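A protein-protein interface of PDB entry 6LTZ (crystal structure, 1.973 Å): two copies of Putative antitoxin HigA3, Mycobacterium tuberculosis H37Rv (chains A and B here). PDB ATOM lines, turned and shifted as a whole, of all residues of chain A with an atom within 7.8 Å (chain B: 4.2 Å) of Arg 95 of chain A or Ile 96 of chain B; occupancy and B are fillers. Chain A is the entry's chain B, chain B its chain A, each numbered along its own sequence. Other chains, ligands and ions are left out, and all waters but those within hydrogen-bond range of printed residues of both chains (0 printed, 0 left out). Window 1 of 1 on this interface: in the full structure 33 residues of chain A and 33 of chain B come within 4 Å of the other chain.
The backbone NH of Leu 80 of chain B lies within hydrogen-bond range of the backbone carbonyl oxygen of Thr 78 of chain A.
The side-chain carboxylate (OE1) of Glu 99 of chain B is in salt-bridge range of the guanidinium group (NH1) of Arg 95 of chain A (3.7 Å).
OE2 of Glu 99 of chain B is in hydrogen-bond range of NE2 of His 93 of chain A, at 2.6 Å.
The backbone NH of Ala 38 of chain A is in hydrogen-bond range of the backbone carbonyl oxygen of Glu 106 of chain B.
The backbone NH (N) of Arg 95 of chain B is in hydrogen-bond range of the backbone carbonyl oxygen (O) of Val 97 of chain A.
O of Val 36 of chain A sits at hydrogen-bond distance from N of Glu 106 of chain B.
N of Arg 95 of chain A lies within hydrogen-bond range of O of Val 97 of chain B (2.8 Å).
O of Ile 96 of chain B lies within hydrogen-bond range of N of Leu 107 of chain B, 3.0 Å away.
O of Leu 75 of chain A sits close to OG1 of Thr 78 of chain A (3.4 Å).
O of Val 87 of chain A sits at hydrogen-bond distance from N of Gly 92 of chain A, at 3.0 Å.
The guanidinium group (NH2) of Arg 95 of chain B lies within salt-bridge range of the side-chain carboxylate (OE1) of Glu 106 of chain B, at 2.6 Å.
OE2 of Glu 106 of chain A is in salt-bridge range of NE of Arg 95 of chain A (3.5 Å).
The backbone NH (N) of Leu 107 of chain A is in hydrogen-bond range of the backbone carbonyl oxygen (O) of Ile 96 of chain A, at 2.9 Å.
Among the printed residues, merely in contact across the chains: Gly 92 of chain A with Glu 99 of chain B, Leu 75 of chain A with Leu 80 of chain B, Ala 38 of chain A with Leu 107 of chain B, Arg 95 of chain A with Ile 96 of chain B, Leu 94 of chain A with Ile 96 of chain B, Leu 94 of chain A with Val 97 of chain B, Ile 96 of chain A with Arg 95 of chain B, Leu 83 of chain A with Leu 107 of chain B, Ile 44 of chain A with Leu 107 of chain B, His 93 of chain A with Val 97 of chain B, Arg 95 of chain A with Arg 95 of chain B, Leu 83 of chain A with Leu 80 of chain B, Leu 75 of chain A with Leu 107 of chain B and Leu 80 of chain A with Leu 80 of chain B.
Of the printed residues of chain B, Val 36 of chain A touches Glu 106 (2.9 Å).
Of the printed residues of chain B, Ala 38 of chain A touches Glu 106 and Leu 107.
Of the printed residues of chain B, Thr 78 of chain A touches Leu 80.
Of the printed residues of chain B, Leu 83 of chain A touches Leu 80 and Leu 107.
Arg 95 of chain A touches just these residues of chain B: Arg 95, Ile 96, Val 97 and Glu 99.
Of chain A, only Leu 94 and Arg 95 come within 4 Å of Ile 96 of chain B.
Of the printed residues of chain A, Val 97 of chain B touches His 93 (3.8 Å), Leu 94 (3.6 Å) and Arg 95 (2.8 Å).
The nearest printed residue of chain B that does not touch Arg 95 of chain A is Leu 107 of chain B (7.4 Å).
Of the 8 printed residues of chain B, 7 touch a printed residue of chain A.
Hydrophobic or aromatic side chains of chain B within 4 Å of the printed part of chain A: Leu 80, Ile 96 and Leu 107.
Among the printed residues, 21 pairs touch across the chains.
Among the printed residues, Asp or Glu carboxylates within 4 Å of a Lys or Arg side-chain nitrogen of the other chain: Arg 95 of chain A with Glu 99 of chain B.
Leu 80 of chain B touches its own counterpart, Leu 80 of chain A.
Arg 95 of chain A touches its own counterpart, Arg 95 of chain B.
Arg 95 of chain A touches Ile 96 of chain B, and with the chains exchanged Ile 96 of chain A touches Arg 95 of chain B.
Arg 95 of chain A touches Val 97 of chain B, and with the chains exchanged Val 97 of chain A touches Arg 95 of chain B.
Positions printed for both chains: 80, 95, 96, 97, 106 and 107.
Of the 21 pairs that touch across the chains among the printed residues, 6 have their exchanged pair printed and touching as well.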
ATOM      1  N   VAL A  36     -24.681  -9.369 -15.297  1.00  0.00           N
ATOM      2  CA  VAL A  36     -23.248  -9.166 -15.157  1.00  0.00           C
ATOM      3  C   VAL A  36     -22.644  -9.293 -16.552  1.00  0.00           C
ATOM      4  O   VAL A  36     -23.220  -9.949 -17.421  1.00  0.00           O
ATOM      5  CB  VAL A  36     -22.599 -10.176 -14.180  1.00  0.00           C
ATOM      6  CG1 VAL A  36     -23.556 -10.509 -13.047  1.00  0.00           C
ATOM      7  CG2 VAL A  36     -22.164 -11.440 -14.900  1.00  0.00           C
ATOM      8  N   ALA A  38     -19.686 -10.469 -19.228  1.00  0.00           N
ATOM      9  CA  ALA A  38     -18.600 -11.417 -19.431  1.00  0.00           C
ATOM     10  C   ALA A  38     -17.851 -11.108 -20.720  1.00  0.00           C
ATOM     11  O   ALA A  38     -18.434 -11.111 -21.804  1.00  0.00           O
ATOM     12  CB  ALA A  38     -19.133 -12.848 -19.454  1.00  0.00           C
ATOM     13  N   ILE A  44     -18.431 -16.334 -17.469  1.00  0.00           N
ATOM     14  CA  ILE A  44     -19.811 -16.810 -17.421  1.00  0.00           C
ATOM     15  C   ILE A  44     -19.975 -17.792 -16.265  1.00  0.00           C
ATOM     16  O   ILE A  44     -20.882 -17.670 -15.438  1.00  0.00           O
ATOM     17  CB  ILE A  44     -20.224 -17.491 -18.734  1.00  0.00           C
ATOM     18  CG1 ILE A  44     -20.051 -16.528 -19.911  1.00  0.00           C
ATOM     19  CG2 ILE A  44     -21.654 -17.985 -18.636  1.00  0.00           C
ATOM     20  CD1 ILE A  44     -20.357 -17.154 -21.262  1.00  0.00           C
ATOM     21  N   LEU A  75     -13.370 -15.080 -26.813  1.00  0.00           N
ATOM     22  CA  LEU A  75     -14.802 -15.311 -26.927  1.00  0.00           C
ATOM     23  C   LEU A  75     -15.253 -15.200 -28.388  1.00  0.00           C
ATOM     24  O   LEU A  75     -16.111 -15.957 -28.843  1.00  0.00           O
ATOM     25  CB  LEU A  75     -15.560 -14.321 -26.042  1.00  0.00           C
ATOM     26  CG  LEU A  75     -16.966 -14.669 -25.559  1.00  0.00           C
ATOM     27  CD1 LEU A  75     -17.054 -16.118 -25.083  1.00  0.00           C
ATOM     28  CD2 LEU A  75     -17.372 -13.714 -24.441  1.00  0.00           C
ATOM     29  N   THR A  78     -14.830 -18.419 -30.340  1.00  0.00           N
ATOM     30  CA  THR A  78     -15.563 -19.566 -29.812  1.00  0.00           C
ATOM     31  C   THR A  78     -16.726 -19.932 -30.733  1.00  0.00           C
ATOM     32  O   THR A  78     -17.454 -19.055 -31.200  1.00  0.00           O
ATOM     33  CB  THR A  78     -16.103 -19.276 -28.402  1.00  0.00           C
ATOM     34  OG1 THR A  78     -15.022 -18.878 -27.548  1.00  0.00           O
ATOM     35  CG2 THR A  78     -16.790 -20.510 -27.817  1.00  0.00           C
ATOM     36  N   LEU A  80     -20.394 -21.322 -31.821  1.00  0.00           N
ATOM     37  CA  LEU A  80     -21.716 -21.188 -31.218  1.00  0.00           C
ATOM     38  C   LEU A  80     -22.193 -22.472 -30.546  1.00  0.00           C
ATOM     39  O   LEU A  80     -22.810 -22.428 -29.485  1.00  0.00           O
ATOM     40  CB  LEU A  80     -22.733 -20.760 -32.271  1.00  0.00           C
ATOM     41  CG  LEU A  80     -24.138 -20.516 -31.726  1.00  0.00           C
ATOM     42  CD1 LEU A  80     -24.114 -19.358 -30.733  1.00  0.00           C
ATOM     43  CD2 LEU A  80     -25.124 -20.263 -32.859  1.00  0.00           C
ATOM     44  N   LEU A  83     -20.400 -22.761 -27.231  1.00  0.00           N
ATOM     45  CA  LEU A  83     -20.973 -21.820 -26.277  1.00  0.00           C
ATOM     46  C   LEU A  83     -22.307 -22.343 -25.752  1.00  0.00           C
ATOM     47  O   LEU A  83     -22.593 -22.264 -24.561  1.00  0.00           O
ATOM     48  CB  LEU A  83     -21.163 -20.442 -26.923  1.00  0.00           C
ATOM     49  CG  LEU A  83     -21.853 -19.411 -26.025  1.00  0.00           C
ATOM     50  CD1 LEU A  83     -20.994 -19.093 -24.808  1.00  0.00           C
ATOM     51  CD2 LEU A  83     -22.198 -18.142 -26.804  1.00  0.00           C
ATOM     52  N   VAL A  87     -23.008 -23.164 -21.773  1.00  0.00           N
ATOM     53  CA  VAL A  87     -24.069 -22.533 -21.011  1.00  0.00           C
ATOM     54  C   VAL A  87     -25.087 -23.575 -20.539  1.00  0.00           C
ATOM     55  O   VAL A  87     -25.606 -23.473 -19.427  1.00  0.00           O
ATOM     56  CB  VAL A  87     -24.757 -21.421 -21.842  1.00  0.00           C
ATOM     57  CG1 VAL A  87     -26.015 -20.926 -21.163  1.00  0.00           C
ATOM     58  CG2 VAL A  87     -23.775 -20.266 -22.071  1.00  0.00           C
ATOM     59  N   GLY A  92     -28.115 -23.071 -17.813  1.00  0.00           N
ATOM     60  CA  GLY A  92     -28.780 -21.949 -18.455  1.00  0.00           C
ATOM     61  C   GLY A  92     -29.111 -22.202 -19.914  1.00  0.00           C
ATOM     62  O   GLY A  92     -28.964 -23.312 -20.416  1.00  0.00           O
ATOM     63  N   HIS A  93     -29.574 -21.163 -20.596  1.00  0.00           N
ATOM     64  CA  HIS A  93     -29.795 -21.252 -22.031  1.00  0.00           C
ATOM     65  C   HIS A  93     -29.358 -19.960 -22.704  1.00  0.00           C
ATOM     66  O   HIS A  93     -29.286 -18.907 -22.070  1.00  0.00           O
ATOM     67  CB  HIS A  93     -31.261 -21.554 -22.344  1.00  0.00           C
ATOM     68  CG  HIS A  93     -32.205 -20.461 -21.952  1.00  0.00           C
ATOM     69  ND1 HIS A  93     -32.693 -20.324 -20.670  1.00  0.00           N
ATOM     70  CD2 HIS A  93     -32.756 -19.456 -22.674  1.00  0.00           C
ATOM     71  CE1 HIS A  93     -33.503 -19.280 -20.619  1.00  0.00           C
ATOM     72  NE2 HIS A  93     -33.557 -18.735 -21.822  1.00  0.00           N
ATOM     73  N   LEU A  94     -29.043 -20.056 -23.988  1.00  0.00           N
ATOM     74  CA  LEU A  94     -28.627 -18.895 -24.765  1.00  0.00           C
ATOM     75  C   LEU A  94     -29.813 -18.122 -25.314  1.00  0.00           C
ATOM     76  O   LEU A  94     -30.741 -18.710 -25.867  1.00  0.00           O
ATOM     77  CB  LEU A  94     -27.737 -19.317 -25.933  1.00  0.00           C
ATOM     78  CG  LEU A  94     -26.240 -19.512 -25.724  1.00  0.00           C
ATOM     79  CD1 LEU A  94     -25.596 -19.876 -27.055  1.00  0.00           C
ATOM     80  CD2 LEU A  94     -25.610 -18.251 -25.150  1.00  0.00           C
ATOM     81  N   ARG A  95     -29.780 -16.805 -25.158  1.00  0.00           N
ATOM     82  CA  ARG A  95     -30.628 -15.939 -25.962  1.00  0.00           C
ATOM     83  C   ARG A  95     -29.731 -15.170 -26.923  1.00  0.00           C
ATOM     84  O   ARG A  95     -28.846 -14.421 -26.501  1.00  0.00           O
ATOM     85  CB  ARG A  95     -31.456 -14.985 -25.097  1.00  0.00           C
ATOM     86  CG  ARG A  95     -32.945 -15.315 -25.111  1.00  0.00           C
ATOM     87  CD  ARG A  95     -33.782 -14.324 -24.313  1.00  0.00           C
ATOM     88  NE  ARG A  95     -34.168 -13.148 -25.087  1.00  0.00           N
ATOM     89  CZ  ARG A  95     -33.687 -11.924 -24.882  1.00  0.00           C
ATOM     90  NH1 ARG A  95     -32.797 -11.709 -23.923  1.00  0.00           N
ATOM     91  NH2 ARG A  95     -34.105 -10.914 -25.634  1.00  0.00           N
ATOM     92  N   ILE A  96     -29.947 -15.391 -28.217  1.00  0.00           N
ATOM     93  CA  ILE A  96     -29.179 -14.716 -29.253  1.00  0.00           C
ATOM     94  C   ILE A  96     -30.057 -13.689 -29.939  1.00  0.00           C
ATOM     95  O   ILE A  96     -31.024 -14.031 -30.620  1.00  0.00           O
ATOM     96  CB  ILE A  96     -28.628 -15.703 -30.292  1.00  0.00           C
ATOM     97  CG1 ILE A  96     -27.746 -16.749 -29.608  1.00  0.00           C
ATOM     98  CG2 ILE A  96     -27.843 -14.958 -31.363  1.00  0.00           C
ATOM     99  CD1 ILE A  96     -27.390 -17.903 -30.501  1.00  0.00           C
ATOM    100  N   VAL A  97     -29.713 -12.425 -29.743  1.00  0.00           N
ATOM    101  CA  VAL A  97     -30.551 -11.327 -30.176  1.00  0.00           C
ATOM    102  C   VAL A  97     -29.793 -10.421 -31.131  1.00  0.00           C
ATOM    103  O   VAL A  97     -28.593 -10.199 -30.979  1.00  0.00           O
ATOM    104  CB  VAL A  97     -31.068 -10.531 -28.954  1.00  0.00           C
ATOM    105  CG1 VAL A  97     -31.382  -9.089 -29.307  1.00  0.00           C
ATOM    106  CG2 VAL A  97     -32.282 -11.228 -28.358  1.00  0.00           C
ATOM    107  N   ALA A  98     -30.493  -9.930 -32.142  1.00  0.00           N
ATOM    108  CA  ALA A  98     -29.934  -8.915 -33.010  1.00  0.00           C
ATOM    109  C   ALA A  98     -30.818  -7.673 -32.971  1.00  0.00           C
ATOM    110  O   ALA A  98     -32.007  -7.724 -33.298  1.00  0.00           O
ATOM    111  CB  ALA A  98     -29.794  -9.446 -34.412  1.00  0.00           C
ATOM    112  N   THR A 104     -35.850  -5.701 -31.978  1.00  0.00           N
ATOM    113  CA  THR A 104     -34.901  -6.809 -31.718  1.00  0.00           C
ATOM    114  C   THR A 104     -35.472  -8.078 -32.343  1.00  0.00           C
ATOM    115  O   THR A 104     -36.652  -8.339 -32.116  1.00  0.00           O
ATOM    116  CB  THR A 104     -34.700  -7.068 -30.223  1.00  0.00           C
ATOM    117  OG1 THR A 104     -35.803  -7.842 -29.762  1.00  0.00           O
ATOM    118  CG2 THR A 104     -34.560  -5.825 -29.374  1.00  0.00           C
ATOM    119  N   VAL A 105     -34.656  -8.838 -33.055  1.00  0.00           N
ATOM    120  CA  VAL A 105     -35.087 -10.125 -33.667  1.00  0.00           C
ATOM    121  C   VAL A 105     -34.380 -11.257 -32.908  1.00  0.00           C
ATOM    122  O   VAL A 105     -33.207 -11.120 -32.636  1.00  0.00           O
ATOM    123  CB  VAL A 105     -34.721 -10.141 -35.160  1.00  0.00           C
ATOM    124  CG1 VAL A 105     -34.345 -11.521 -35.654  1.00  0.00           C
ATOM    125  CG2 VAL A 105     -35.803  -9.534 -36.026  1.00  0.00           C
ATOM    126  N   GLU A 106     -35.070 -12.345 -32.601  1.00  0.00           N
ATOM    127  CA  GLU A 106     -34.419 -13.444 -31.853  1.00  0.00           C
ATOM    128  C   GLU A 106     -34.020 -14.545 -32.830  1.00  0.00           C
ATOM    129  O   GLU A 106     -34.866 -14.951 -33.600  1.00  0.00           O
ATOM    130  CB  GLU A 106     -35.387 -13.993 -30.811  1.00  0.00           C
ATOM    131  CG  GLU A 106     -34.868 -15.232 -30.131  1.00  0.00           C
ATOM    132  CD  GLU A 106     -35.198 -15.332 -28.658  1.00  0.00           C
ATOM    133  OE1 GLU A 106     -35.108 -16.422 -28.125  1.00  0.00           O
ATOM    134  OE2 GLU A 106     -35.523 -14.313 -28.060  1.00  0.00           O
ATOM    135  N   LEU A 107     -32.766 -14.982 -32.798  1.00  0.00           N
ATOM    136  CA  LEU A 107     -32.308 -16.040 -33.731  1.00  0.00           C
ATOM    137  C   LEU A 107     -32.590 -17.393 -33.083  1.00  0.00           C
ATOM    138  O   LEU A 107     -32.200 -17.577 -31.931  1.00  0.00           O
ATOM    139  CB  LEU A 107     -30.833 -15.830 -34.092  1.00  0.00           C
ATOM    140  CG  LEU A 107     -30.255 -14.427 -33.858  1.00  0.00           C
ATOM    141  CD1 LEU A 107     -28.933 -14.230 -34.582  1.00  0.00           C
ATOM    142  CD2 LEU A 107     -31.202 -13.315 -34.268  1.00  0.00           C
ATOM    143  N   LEU B  80     -18.487 -16.920 -32.923  1.00  0.00           N
ATOM    144  CA  LEU B  80     -19.274 -15.772 -32.474  1.00  0.00           C
ATOM    145  C   LEU B  80     -18.955 -14.518 -33.281  1.00  0.00           C
ATOM    146  O   LEU B  80     -19.856 -13.773 -33.666  1.00  0.00           O
ATOM    147  CB  LEU B  80     -19.029 -15.501 -30.989  1.00  0.00           C
ATOM    148  CG  LEU B  80     -19.979 -16.144 -29.978  1.00  0.00           C
ATOM    149  CD1 LEU B  80     -20.335 -17.569 -30.359  1.00  0.00           C
ATOM    150  CD2 LEU B  80     -19.396 -16.088 -28.564  1.00  0.00           C
ATOM    151  N   ARG B  95     -26.392  -9.221 -29.852  1.00  0.00           N
ATOM    152  CA  ARG B  95     -26.254  -9.398 -28.410  1.00  0.00           C
ATOM    153  C   ARG B  95     -26.469 -10.858 -28.064  1.00  0.00           C
ATOM    154  O   ARG B  95     -27.369 -11.507 -28.594  1.00  0.00           O
ATOM    155  CB  ARG B  95     -27.240  -8.517 -27.638  1.00  0.00           C
ATOM    156  CG  ARG B  95     -26.927  -7.032 -27.720  1.00  0.00           C
ATOM    157  CD  ARG B  95     -28.020  -6.188 -27.083  1.00  0.00           C
ATOM    158  NE  ARG B  95     -27.945  -6.171 -25.624  1.00  0.00           N
ATOM    159  CZ  ARG B  95     -28.923  -6.578 -24.821  1.00  0.00           C
ATOM    160  NH1 ARG B  95     -30.058  -7.035 -25.332  1.00  0.00           N
ATOM    161  NH2 ARG B  95     -28.767  -6.522 -23.505  1.00  0.00           N
ATOM    162  N   ILE B  96     -25.618 -11.373 -27.184  1.00  0.00           N
ATOM    163  CA  ILE B  96     -25.759 -12.736 -26.700  1.00  0.00           C
ATOM    164  C   ILE B  96     -25.859 -12.708 -25.185  1.00  0.00           C
ATOM    165  O   ILE B  96     -25.023 -12.124 -24.497  1.00  0.00           O
ATOM    166  CB  ILE B  96     -24.591 -13.623 -27.129  1.00  0.00           C
ATOM    167  CG1 ILE B  96     -24.548 -13.724 -28.655  1.00  0.00           C
ATOM    168  CG2 ILE B  96     -24.721 -15.021 -26.512  1.00  0.00           C
ATOM    169  CD1 ILE B  96     -23.397 -14.535 -29.178  1.00  0.00           C
ATOM    170  N   VAL B  97     -26.907 -13.335 -24.681  1.00  0.00           N
ATOM    171  CA  VAL B  97     -27.176 -13.341 -23.259  1.00  0.00           C
ATOM    172  C   VAL B  97     -27.274 -14.780 -22.774  1.00  0.00           C
ATOM    173  O   VAL B  97     -28.001 -15.588 -23.354  1.00  0.00           O
ATOM    174  CB  VAL B  97     -28.477 -12.575 -22.942  1.00  0.00           C
ATOM    175  CG1 VAL B  97     -28.939 -12.870 -21.540  1.00  0.00           C
ATOM    176  CG2 VAL B  97     -28.276 -11.075 -23.149  1.00  0.00           C
ATOM    177  N   GLU B  99     -28.813 -16.901 -20.106  1.00  0.00           N
ATOM    178  CA  GLU B  99     -29.880 -16.727 -19.131  1.00  0.00           C
ATOM    179  C   GLU B  99     -29.864 -17.831 -18.083  1.00  0.00           C
ATOM    180  O   GLU B  99     -29.919 -19.011 -18.414  1.00  0.00           O
ATOM    181  CB  GLU B  99     -31.234 -16.670 -19.830  1.00  0.00           C
ATOM    182  CG  GLU B  99     -31.387 -15.449 -20.720  1.00  0.00           C
ATOM    183  CD  GLU B  99     -32.817 -15.220 -21.156  1.00  0.00           C
ATOM    184  OE1 GLU B  99     -33.265 -14.054 -21.126  1.00  0.00           O
ATOM    185  OE2 GLU B  99     -33.492 -16.202 -21.529  1.00  0.00           O
ATOM    186  N   GLU B 106     -24.450 -11.211 -19.730  1.00  0.00           N
ATOM    187  CA  GLU B 106     -24.346 -10.758 -21.112  1.00  0.00           C
ATOM    188  C   GLU B 106     -22.903 -10.799 -21.585  1.00  0.00           C
ATOM    189  O   GLU B 106     -21.991 -10.334 -20.903  1.00  0.00           O
ATOM    190  CB  GLU B 106     -24.917  -9.350 -21.287  1.00  0.00           C
ATOM    191  CG  GLU B 106     -24.642  -8.775 -22.668  1.00  0.00           C
ATOM    192  CD  GLU B 106     -25.735  -7.847 -23.156  1.00  0.00           C
ATOM    193  OE1 GLU B 106     -26.592  -7.453 -22.339  1.00  0.00           O
ATOM    194  OE2 GLU B 106     -25.731  -7.513 -24.362  1.00  0.00           O
ATOM    195  N   LEU B 107     -22.705 -11.374 -22.762  1.00  0.00           N
ATOM    196  CA  LEU B 107     -21.380 -11.483 -23.347  1.00  0.00           C
ATOM    197  C   LEU B 107     -21.011 -10.188 -24.055  1.00  0.00           C
ATOM    198  O   LEU B 107     -21.840  -9.586 -24.734  1.00  0.00           O
ATOM    199  CB  LEU B 107     -21.316 -12.654 -24.331  1.00  0.00           C
ATOM    200  CG  LEU B 107     -21.227 -14.086 -23.795  1.00  0.00           C
ATOM    201  CD1 LEU B 107     -22.415 -14.455 -22.921  1.00  0.00           C
ATOM    202  CD2 LEU B 107     -21.105 -15.062 -24.957  1.00  0.00           C
ATOM    203  N   LEU B 110     -17.682  -9.528 -28.580  1.00  0.00           N
ATOM    204  CA  LEU B 110     -18.044 -10.554 -29.555  1.00  0.00           C
ATOM    205  C   LEU B 110     -17.380 -10.320 -30.906  1.00  0.00           C
ATOM    206  O   LEU B 110     -17.370 -11.205 -31.760  1.00  0.00           O
ATOM    207  CB  LEU B 110     -19.561 -10.616 -29.728  1.00  0.00           C
ATOM    208  CG  LEU B 110     -20.378 -11.513 -28.794  1.00  0.00           C
ATOM    209  CD1 LEU B 110     -19.588 -11.964 -27.574  1.00  0.00           C
ATOM    210  CD2 LEU B 110     -21.678 -10.828 -28.397  1.00  0.00           C
